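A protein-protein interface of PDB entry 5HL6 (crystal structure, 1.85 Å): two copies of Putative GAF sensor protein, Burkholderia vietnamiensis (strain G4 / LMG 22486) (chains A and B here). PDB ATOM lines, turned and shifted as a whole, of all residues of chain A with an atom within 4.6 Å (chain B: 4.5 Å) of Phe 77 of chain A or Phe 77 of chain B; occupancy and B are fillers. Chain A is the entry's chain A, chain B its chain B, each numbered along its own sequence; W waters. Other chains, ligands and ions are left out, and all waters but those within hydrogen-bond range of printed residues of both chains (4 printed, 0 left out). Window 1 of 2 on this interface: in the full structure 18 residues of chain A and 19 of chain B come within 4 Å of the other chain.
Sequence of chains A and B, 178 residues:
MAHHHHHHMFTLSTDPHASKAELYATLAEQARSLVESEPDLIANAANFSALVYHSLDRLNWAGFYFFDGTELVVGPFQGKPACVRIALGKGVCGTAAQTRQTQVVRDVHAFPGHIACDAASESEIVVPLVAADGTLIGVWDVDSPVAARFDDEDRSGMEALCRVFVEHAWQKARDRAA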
ATOM      1  N   ALA A  46     -11.332  -4.052   8.669  1.00  0.00           N
ATOM      2  CA  ALA A  46     -12.538  -3.466   9.253  1.00  0.00           C
ATOM      3  C   ALA A  46     -13.118  -2.365   8.358  1.00  0.00           C
ATOM      4  O   ALA A  46     -14.340  -2.299   8.155  1.00  0.00           O
ATOM      5  CB  ALA A  46     -12.232  -2.940  10.657  1.00  0.00           C
ATOM      6  N   ASN A  47     -12.259  -1.515   7.787  1.00  0.00           N
ATOM      7  CA  ASN A  47     -12.748  -0.437   6.927  1.00  0.00           C
ATOM      8  C   ASN A  47     -13.309  -0.978   5.621  1.00  0.00           C
ATOM      9  O   ASN A  47     -14.321  -0.480   5.124  1.00  0.00           O
ATOM     10  CB  ASN A  47     -11.630   0.555   6.641  1.00  0.00           C
ATOM     11  CG  ASN A  47     -11.433   1.523   7.782  1.00  0.00           C
ATOM     12  OD1 ASN A  47     -12.398   1.898   8.438  1.00  0.00           O
ATOM     13  ND2 ASN A  47     -10.184   1.910   8.043  1.00  0.00           N
ATOM     14  N   SER A  49     -14.754  -3.934   5.220  1.00  0.00           N
ATOM     15  CA  SER A  49     -16.072  -4.486   5.539  1.00  0.00           C
ATOM     16  C   SER A  49     -17.110  -3.385   5.689  1.00  0.00           C
ATOM     17  O   SER A  49     -18.237  -3.509   5.195  1.00  0.00           O
ATOM     18  CB  SER A  49     -16.019  -5.327   6.825  1.00  0.00           C
ATOM     19  OG  SER A  49     -15.028  -6.317   6.713  1.00  0.00           O
ATOM     20  N   ALA A  50     -16.750  -2.300   6.380  1.00  0.00           N
ATOM     21  CA  ALA A  50     -17.678  -1.185   6.526  1.00  0.00           C
ATOM     22  C   ALA A  50     -17.993  -0.540   5.182  1.00  0.00           C
ATOM     23  O   ALA A  50     -19.138  -0.152   4.931  1.00  0.00           O
ATOM     24  CB  ALA A  50     -17.106  -0.150   7.497  1.00  0.00           C
ATOM     25  N   TRP A  61     -24.842  -9.160   6.459  1.00  0.00           N
ATOM     26  CA  TRP A  61     -23.534  -9.507   6.999  1.00  0.00           C
ATOM     27  C   TRP A  61     -22.490  -9.302   5.912  1.00  0.00           C
ATOM     28  O   TRP A  61     -22.747  -9.592   4.743  1.00  0.00           O
ATOM     29  CB  TRP A  61     -23.524 -10.958   7.497  1.00  0.00           C
ATOM     30  CG  TRP A  61     -22.596 -11.249   8.640  1.00  0.00           C
ATOM     31  CD1 TRP A  61     -22.909 -11.231   9.971  1.00  0.00           C
ATOM     32  CD2 TRP A  61     -21.226 -11.653   8.557  1.00  0.00           C
ATOM     33  NE1 TRP A  61     -21.812 -11.580  10.719  1.00  0.00           N
ATOM     34  CE2 TRP A  61     -20.768 -11.853   9.876  1.00  0.00           C
ATOM     35  CE3 TRP A  61     -20.342 -11.872   7.495  1.00  0.00           C
ATOM     36  CZ2 TRP A  61     -19.466 -12.260  10.160  1.00  0.00           C
ATOM     37  CZ3 TRP A  61     -19.048 -12.265   7.779  1.00  0.00           C
ATOM     38  CH2 TRP A  61     -18.619 -12.455   9.101  1.00  0.00           C
ATOM     39  N   ALA A  62     -21.324  -8.789   6.295  1.00  0.00           N
ATOM     40  CA  ALA A  62     -20.210  -8.652   5.356  1.00  0.00           C
ATOM     41  C   ALA A  62     -18.923  -8.651   6.162  1.00  0.00           C
ATOM     42  O   ALA A  62     -18.763  -7.808   7.051  1.00  0.00           O
ATOM     43  CB  ALA A  62     -20.327  -7.359   4.523  1.00  0.00           C
ATOM     44  N   GLY A  63     -18.008  -9.570   5.873  1.00  0.00           N
ATOM     45  CA  GLY A  63     -16.796  -9.612   6.671  1.00  0.00           C
ATOM     46  C   GLY A  63     -15.863 -10.747   6.299  1.00  0.00           C
ATOM     47  O   GLY A  63     -16.100 -11.507   5.347  1.00  0.00           O
ATOM     48  N   PHE A  64     -14.803 -10.861   7.105  1.00  0.00           N
ATOM     49  CA  PHE A  64     -13.672 -11.738   6.837  1.00  0.00           C
ATOM     50  C   PHE A  64     -13.620 -12.895   7.826  1.00  0.00           C
ATOM     51  O   PHE A  64     -13.942 -12.732   9.011  1.00  0.00           O
ATOM     52  CB  PHE A  64     -12.348 -10.969   6.920  1.00  0.00           C
ATOM     53  CG  PHE A  64     -12.119  -9.985   5.786  1.00  0.00           C
ATOM     54  CD1 PHE A  64     -11.474 -10.397   4.624  1.00  0.00           C
ATOM     55  CD2 PHE A  64     -12.531  -8.655   5.891  1.00  0.00           C
ATOM     56  CE1 PHE A  64     -11.249  -9.512   3.580  1.00  0.00           C
ATOM     57  CE2 PHE A  64     -12.314  -7.764   4.857  1.00  0.00           C
ATOM     58  CZ  PHE A  64     -11.667  -8.185   3.694  1.00  0.00           C
ATOM     59  N   VAL A  74     -13.201 -15.993  12.603  1.00  0.00           N
ATOM     60  CA  VAL A  74     -13.772 -14.720  12.166  1.00  0.00           C
ATOM     61  C   VAL A  74     -12.824 -13.564  12.467  1.00  0.00           C
ATOM     62  O   VAL A  74     -12.171 -13.516  13.523  1.00  0.00           O
ATOM     63  CB  VAL A  74     -15.161 -14.495  12.793  1.00  0.00           C
ATOM     64  CG1 VAL A  74     -15.070 -14.082  14.288  1.00  0.00           C
ATOM     65  CG2 VAL A  74     -15.945 -13.454  11.958  1.00  0.00           C
ATOM     66  N   GLY A  75     -12.739 -12.622  11.512  1.00  0.00           N
ATOM     67  CA  GLY A  75     -12.019 -11.383  11.665  1.00  0.00           C
ATOM     68  C   GLY A  75     -13.003 -10.219  11.703  1.00  0.00           C
ATOM     69  O   GLY A  75     -14.170 -10.404  12.057  1.00  0.00           O
ATOM     70  N   PRO A  76     -12.579  -9.013  11.325  1.00  0.00           N
ATOM     71  CA  PRO A  76     -13.527  -7.885  11.324  1.00  0.00           C
ATOM     72  C   PRO A  76     -14.715  -8.174  10.415  1.00  0.00           C
ATOM     73  O   PRO A  76     -14.568  -8.779   9.349  1.00  0.00           O
ATOM     74  CB  PRO A  76     -12.687  -6.709  10.807  1.00  0.00           C
ATOM     75  CG  PRO A  76     -11.265  -7.085  11.218  1.00  0.00           C
ATOM     76  CD  PRO A  76     -11.208  -8.579  11.004  1.00  0.00           C
ATOM     77  N   PHE A  77     -15.901  -7.746  10.851  1.00  0.00           N
ATOM     78  CA  PHE A  77     -17.112  -7.943  10.058  1.00  0.00           C
ATOM     79  C   PHE A  77     -18.160  -6.913  10.466  1.00  0.00           C
ATOM     80  O   PHE A  77     -18.100  -6.345  11.562  1.00  0.00           O
ATOM     81  CB  PHE A  77     -17.677  -9.363  10.226  1.00  0.00           C
ATOM     82  CG  PHE A  77     -18.242  -9.647  11.615  1.00  0.00           C
ATOM     83  CD1 PHE A  77     -19.581  -9.426  11.897  1.00  0.00           C
ATOM     84  CD2 PHE A  77     -17.434 -10.163  12.621  1.00  0.00           C
ATOM     85  CE1 PHE A  77     -20.106  -9.700  13.161  1.00  0.00           C
ATOM     86  CE2 PHE A  77     -17.950 -10.436  13.887  1.00  0.00           C
ATOM     87  CZ  PHE A  77     -19.281 -10.193  14.162  1.00  0.00           C
ATOM     88  N   GLN A  78     -19.141  -6.707   9.582  1.00  0.00           N
ATOM     89  CA  GLN A  78     -20.349  -5.955   9.893  1.00  0.00           C
ATOM     90  C   GLN A  78     -21.549  -6.897   9.943  1.00  0.00           C
ATOM     91  O   GLN A  78     -21.698  -7.776   9.090  1.00  0.00           O
ATOM     92  CB  GLN A  78     -20.587  -4.846   8.849  1.00  0.00           C
ATOM     93  CG  GLN A  78     -19.449  -3.850   8.740  1.00  0.00           C
ATOM     94  CD  GLN A  78     -19.670  -2.610   9.590  1.00  0.00           C
ATOM     95  OE1 GLN A  78     -20.807  -2.205   9.834  1.00  0.00           O
ATOM     96  NE2 GLN A  78     -18.584  -1.996  10.034  1.00  0.00           N
ATOM     97  N   GLY A  79     -22.414  -6.713  10.951  1.00  0.00           N
ATOM     98  CA  GLY A  79     -23.600  -7.534  11.108  1.00  0.00           C
ATOM     99  C   GLY A  79     -23.731  -8.051  12.530  1.00  0.00           C
ATOM    100  O   GLY A  79     -23.035  -7.608  13.450  1.00  0.00           O
ATOM    101  N   LYS A  80     -24.644  -9.002  12.727  1.00  0.00           N
ATOM    102  CA  LYS A  80     -24.806  -9.597  14.043  1.00  0.00           C
ATOM    103  C   LYS A  80     -23.744 -10.671  14.263  1.00  0.00           C
ATOM    104  O   LYS A  80     -23.199 -11.219  13.300  1.00  0.00           O
ATOM    105  CB  LYS A  80     -26.207 -10.185  14.184  1.00  0.00           C
ATOM    106  N   PRO A  81     -23.411 -10.973  15.521  1.00  0.00           N
ATOM    107  CA  PRO A  81     -22.492 -12.087  15.794  1.00  0.00           C
ATOM    108  C   PRO A  81     -22.916 -13.340  15.034  1.00  0.00           C
ATOM    109  O   PRO A  81     -24.102 -13.644  14.919  1.00  0.00           O
ATOM    110  CB  PRO A  81     -22.612 -12.274  17.314  1.00  0.00           C
ATOM    111  CG  PRO A  81     -22.980 -10.918  17.834  1.00  0.00           C
ATOM    112  CD  PRO A  81     -23.849 -10.293  16.759  1.00  0.00           C
ATOM    113  N   ALA B  46     -14.115  -8.363  17.353  1.00  0.00           N
ATOM    114  CA  ALA B  46     -15.156  -8.249  16.335  1.00  0.00           C
ATOM    115  C   ALA B  46     -16.517  -8.674  16.884  1.00  0.00           C
ATOM    116  O   ALA B  46     -17.529  -7.987  16.675  1.00  0.00           O
ATOM    117  CB  ALA B  46     -14.767  -9.060  15.102  1.00  0.00           C
ATOM    118  N   ASN B  47     -16.558  -9.794  17.611  1.00  0.00           N
ATOM    119  CA  ASN B  47     -17.826 -10.286  18.144  1.00  0.00           C
ATOM    120  C   ASN B  47     -18.370  -9.368  19.229  1.00  0.00           C
ATOM    121  O   ASN B  47     -19.584  -9.140  19.307  1.00  0.00           O
ATOM    122  CB  ASN B  47     -17.655 -11.720  18.680  1.00  0.00           C
ATOM    123  CG  ASN B  47     -17.765 -12.747  17.571  1.00  0.00           C
ATOM    124  OD1 ASN B  47     -18.420 -12.492  16.564  1.00  0.00           O
ATOM    125  ND2 ASN B  47     -17.131 -13.909  17.746  1.00  0.00           N
ATOM    126  N   SER B  49     -17.852  -6.070  19.517  1.00  0.00           N
ATOM    127  CA  SER B  49     -18.415  -4.904  18.836  1.00  0.00           C
ATOM    128  C   SER B  49     -19.799  -5.217  18.285  1.00  0.00           C
ATOM    129  O   SER B  49     -20.739  -4.435  18.455  1.00  0.00           O
ATOM    130  CB  SER B  49     -17.492  -4.445  17.704  1.00  0.00           C
ATOM    131  OG  SER B  49     -16.200  -4.115  18.174  1.00  0.00           O
ATOM    132  N   ALA B  50     -19.944  -6.378  17.633  1.00  0.00           N
ATOM    133  CA  ALA B  50     -21.229  -6.744  17.043  1.00  0.00           C
ATOM    134  C   ALA B  50     -22.296  -6.937  18.113  1.00  0.00           C
ATOM    135  O   ALA B  50     -23.447  -6.521  17.939  1.00  0.00           O
ATOM    136  CB  ALA B  50     -21.080  -8.022  16.213  1.00  0.00           C
ATOM    137  N   TRP B  61     -22.414   3.814  15.779  1.00  0.00           N
ATOM    138  CA  TRP B  61     -21.047   3.323  15.694  1.00  0.00           C
ATOM    139  C   TRP B  61     -20.701   2.673  17.020  1.00  0.00           C
ATOM    140  O   TRP B  61     -21.127   3.157  18.070  1.00  0.00           O
ATOM    141  CB  TRP B  61     -20.058   4.458  15.400  1.00  0.00           C
ATOM    142  CG  TRP B  61     -18.830   4.042  14.622  1.00  0.00           C
ATOM    143  CD1 TRP B  61     -18.697   4.026  13.260  1.00  0.00           C
ATOM    144  CD2 TRP B  61     -17.560   3.620  15.152  1.00  0.00           C
ATOM    145  NE1 TRP B  61     -17.435   3.615  12.912  1.00  0.00           N
ATOM    146  CE2 TRP B  61     -16.717   3.358  14.052  1.00  0.00           C
ATOM    147  CE3 TRP B  61     -17.054   3.443  16.450  1.00  0.00           C
ATOM    148  CZ2 TRP B  61     -15.394   2.948  14.206  1.00  0.00           C
ATOM    149  CZ3 TRP B  61     -15.736   3.013  16.604  1.00  0.00           C
ATOM    150  CH2 TRP B  61     -14.926   2.764  15.488  1.00  0.00           C
ATOM    151  N   ALA B  62     -19.927   1.591  16.965  1.00  0.00           N
ATOM    152  CA  ALA B  62     -19.430   0.963  18.188  1.00  0.00           C
ATOM    153  C   ALA B  62     -18.244   0.079  17.830  1.00  0.00           C
ATOM    154  O   ALA B  62     -18.384  -0.846  17.019  1.00  0.00           O
ATOM    155  CB  ALA B  62     -20.536   0.161  18.874  1.00  0.00           C
ATOM    156  N   GLY B  63     -17.085   0.363  18.415  1.00  0.00           N
ATOM    157  CA  GLY B  63     -15.899  -0.397  18.069  1.00  0.00           C
ATOM    158  C   GLY B  63     -14.669   0.092  18.807  1.00  0.00           C
ATOM    159  O   GLY B  63     -14.733   0.994  19.653  1.00  0.00           O
ATOM    160  N   VAL B  74      -7.632   2.061  14.120  1.00  0.00           N
ATOM    161  CA  VAL B  74      -8.967   1.488  14.266  1.00  0.00           C
ATOM    162  C   VAL B  74      -8.882  -0.033  14.202  1.00  0.00           C
ATOM    163  O   VAL B  74      -8.107  -0.600  13.419  1.00  0.00           O
ATOM    164  CB  VAL B  74      -9.926   2.042  13.199  1.00  0.00           C
ATOM    165  CG1 VAL B  74      -9.612   1.470  11.800  1.00  0.00           C
ATOM    166  CG2 VAL B  74     -11.371   1.747  13.583  1.00  0.00           C
ATOM    167  N   GLY B  75      -9.665  -0.697  15.057  1.00  0.00           N
ATOM    168  CA  GLY B  75      -9.795  -2.145  15.058  1.00  0.00           C
ATOM    169  C   GLY B  75     -11.170  -2.534  14.552  1.00  0.00           C
ATOM    170  O   GLY B  75     -11.784  -1.784  13.792  1.00  0.00           O
ATOM    171  N   PRO B  76     -11.689  -3.707  14.946  1.00  0.00           N
ATOM    172  CA  PRO B  76     -13.048  -4.077  14.526  1.00  0.00           C
ATOM    173  C   PRO B  76     -14.068  -3.059  15.013  1.00  0.00           C
ATOM    174  O   PRO B  76     -13.943  -2.514  16.113  1.00  0.00           O
ATOM    175  CB  PRO B  76     -13.274  -5.448  15.184  1.00  0.00           C
ATOM    176  CG  PRO B  76     -11.903  -5.983  15.477  1.00  0.00           C
ATOM    177  CD  PRO B  76     -11.075  -4.744  15.801  1.00  0.00           C
ATOM    178  N   PHE B  77     -15.095  -2.819  14.193  1.00  0.00           N
ATOM    179  CA  PHE B  77     -16.169  -1.904  14.575  1.00  0.00           C
ATOM    180  C   PHE B  77     -17.416  -2.182  13.742  1.00  0.00           C
ATOM    181  O   PHE B  77     -17.340  -2.750  12.652  1.00  0.00           O
ATOM    182  CB  PHE B  77     -15.734  -0.442  14.407  1.00  0.00           C
ATOM    183  CG  PHE B  77     -15.518  -0.029  12.964  1.00  0.00           C
ATOM    184  CD1 PHE B  77     -16.579   0.427  12.188  1.00  0.00           C
ATOM    185  CD2 PHE B  77     -14.258  -0.099  12.388  1.00  0.00           C
ATOM    186  CE1 PHE B  77     -16.388   0.815  10.858  1.00  0.00           C
ATOM    187  CE2 PHE B  77     -14.063   0.271  11.059  1.00  0.00           C
ATOM    188  CZ  PHE B  77     -15.133   0.731  10.295  1.00  0.00           C
ATOM    189  N   GLN B  78     -18.562  -1.730  14.264  1.00  0.00           N
ATOM    190  CA  GLN B  78     -19.821  -1.623  13.533  1.00  0.00           C
ATOM    191  C   GLN B  78     -20.091  -0.159  13.204  1.00  0.00           C
ATOM    192  O   GLN B  78     -19.890   0.719  14.053  1.00  0.00           O
ATOM    193  CB  GLN B  78     -20.999  -2.170  14.350  1.00  0.00           C
ATOM    194  CG  GLN B  78     -20.796  -3.568  14.873  1.00  0.00           C
ATOM    195  CD  GLN B  78     -20.594  -4.564  13.754  1.00  0.00           C
ATOM    196  OE1 GLN B  78     -21.419  -4.671  12.853  1.00  0.00           O
ATOM    197  NE2 GLN B  78     -19.484  -5.285  13.798  1.00  0.00           N
ATOM    198  N   GLY B  79     -20.551   0.104  11.982  1.00  0.00           N
ATOM    199  CA  GLY B  79     -20.830   1.454  11.528  1.00  0.00           C
ATOM    200  C   GLY B  79     -20.139   1.755  10.215  1.00  0.00           C
ATOM    201  O   GLY B  79     -19.458   0.914   9.628  1.00  0.00           O
ATOM    202  N   LYS B  80     -20.351   2.984   9.731  1.00  0.00           N
ATOM    203  CA  LYS B  80     -19.674   3.423   8.522  1.00  0.00           C
ATOM    204  C   LYS B  80     -18.191   3.660   8.817  1.00  0.00           C
ATOM    205  O   LYS B  80     -17.804   3.809   9.977  1.00  0.00           O
ATOM    206  CB  LYS B  80     -20.336   4.692   7.973  1.00  0.00           C
ATOM    207  N   PRO B  81     -17.336   3.661   7.790  1.00  0.00           N
ATOM    208  CA  PRO B  81     -15.926   4.007   8.008  1.00  0.00           C
ATOM    209  C   PRO B  81     -15.809   5.316   8.781  1.00  0.00           C
ATOM    210  O   PRO B  81     -16.590   6.241   8.574  1.00  0.00           O
ATOM    211  CB  PRO B  81     -15.371   4.139   6.584  1.00  0.00           C
ATOM    212  CG  PRO B  81     -16.246   3.270   5.758  1.00  0.00           C
ATOM    213  CD  PRO B  81     -17.613   3.323   6.380  1.00  0.00           C
HETATM  214  O   HOH W   1     -15.964  -3.120  10.135  1.00  0.00           O
HETATM  215  O   HOH W   2     -17.344  -6.612  14.262  1.00  0.00           O
HETATM  216  O   HOH W   3     -23.405  -3.275  11.426  1.00  0.00           O
HETATM  217  O   HOH W   4     -15.520  -4.980  12.386  1.00  0.00           O
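Asn 47 of chain A touches Phe 77 of chain B, and with the chains exchanged Phe 77 of chain A touches Asn 47 of chain B.
Ala 50 of chain A touches Phe 77 of chain B, and with the chains exchanged Phe 77 of chain A touches Ala 50 of chain B.
Ala 50 of chain A touches Gly 79 of chain B, and with the chains exchanged Gly 79 of chain A touches Ala 50 of chain B.
Phe 77 of chain A touches Gln 78 of chain B, and with the chains exchanged Gln 78 of chain A touches Phe 77 of chain B.
15 positions are printed for both chains.
Of the 19 pairs that touch across the chains among the printed residues, 18 have their exchanged pair printed and touching as well.
The backbone carbonyl oxygen (O) of Phe 77 of chain A sits at hydrogen-bond distance from the side-chain amide nitrogen (NE2) of Gln 78 of chain B (2.8 Å).
The side-chain amide nitrogen (NE2) of Gln 78 of chain A lies within hydrogen-bond range of the backbone carbonyl oxygen (O) of Phe 77 of chain B (3.0 Å).
NE2 of Gln 78 of chain A is in hydrogen-bond range of O of Gly 79 of chain B, at 3.1 Å.
The backbone NH of Gly 79 of chain A lies within hydrogen-bond range of the side-chain amide oxygen of Gln 78 of chain B (3.0 Å).
Of the 16 printed residues of chain A, 8 touch a printed residue of chain B.
Printed residues of chain A that touch a printed residue of chain B: Ala 46, Asn 47, Ala 50, Gly 75, Phe 77, Gln 78, Gly 79 and Pro 81.
Printed residues of chain B that touch a printed residue of chain A: Ala 46, Asn 47, Ala 50, Val 74, Gly 75, Phe 77, Gln 78, Gly 79 and Pro 81.
Hydrophobic or aromatic side chains of chain B within 4 Å of the printed part of chain A: Ala 46, Ala 50, Val 74, Phe 77 and Pro 81.
Among the printed residues, 19 pairs touch across the chains.
Among the printed residues, no Asp or Glu carboxylate lies within 4 Å of a Lys or Arg side-chain nitrogen of the other chain.
O of Ala 62 of chain A sits at hydrogen-bond distance from N of Gln 78 of chain A, at 2.8 Å.
O of Phe 64 of chain A lies within hydrogen-bond range of N of Gly 75 of chain A, at 2.8 Å.
O of Ala 62 of chain B lies within hydrogen-bond range of N of Gln 78 of chain B, 2.9 Å away.
Of chain B, only Ala 46 (3.7 Å), Asn 47 (3.4 Å), Ala 50 (3.5 Å), Phe 77 (3.8 Å) and Gln 78 (2.8 Å) come within 4 Å of Phe 77 of chain A.
Phe 77 of chain B touches just these residues of chain A: Ala 46, Asn 47, Ala 50, Phe 77 and Gln 78.
Of the printed residues of chain B, Gly 75 of chain A touches Ala 46 (3.4 Å).
Printed residues of chain A within 4 Å of Gly 79 of chain B: Ala 50 (3.3 Å) and Gln 78 (3.1 Å).
Of the printed residues of chain A, Asn 47 of chain B touches Phe 77 (3.4 Å).
Printed residues of chain B within 4 Å of Ala 50 of chain A: Phe 77, Gly 79 and Pro 81.
Pro 76 of chain B touches none of the printed residues of chain A.
Among the printed residues, merely in contact across the chains: Ala 46 of chain A with Gly 75 of chain B (3.4 Å), Ala 46 of chain A with Phe 77 of chain B (3.7 Å), Asn 47 of chain A with Val 74 of chain B (3.8 Å), Asn 47 of chain A with Phe 77 of chain B (3.5 Å), Ala 50 of chain A with Phe 77 of chain B (3.5 Å), Ala 50 of chain A with Gly 79 of chain B (3.3 Å), Ala 50 of chain A with Pro 81 of chain B (3.7 Å), Gly 75 of chain A with Ala 46 of chain B (3.4 Å), Phe 77 of chain A with Ala 46 of chain B (3.7 Å), Phe 77 of chain A with Asn 47 of chain B (3.4 Å), Phe 77 of chain A with Ala 50 of chain B (3.5 Å), Phe 77 of chain A with Phe 77 of chain B (3.8 Å), Gln 78 of chain A with Gln 78 of chain B (3.4 Å), Gly 79 of chain A with Ala 50 of chain B (3.4 Å) and Pro 81 of chain A with Ala 50 of chain B (3.6 Å).
Water W2 lies within hydrogen-bond range of NE2 of Gln 78 of chain B, O of Ala 46 of chain B and O of Phe 77 of chain A.
Water W1 lies within hydrogen-bond range of O of Ala 46 of chain A (2.7 Å), NE2 of Gln 78 of chain A (2.9 Å) and O of Phe 77 of chain B (2.9 Å).
Water W3 bridges the side-chain amide oxygen (OE1) of Gln 78 of chain B (2.8 Å) and the side-chain amide oxygen (OE1) of Gln 78 of chain A (3.2 Å).
Water W4 bridges the backbone NH of Phe 77 of chain B (2.8 Å) and the backbone carbonyl oxygen of Phe 77 of chain A (3.0 Å).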
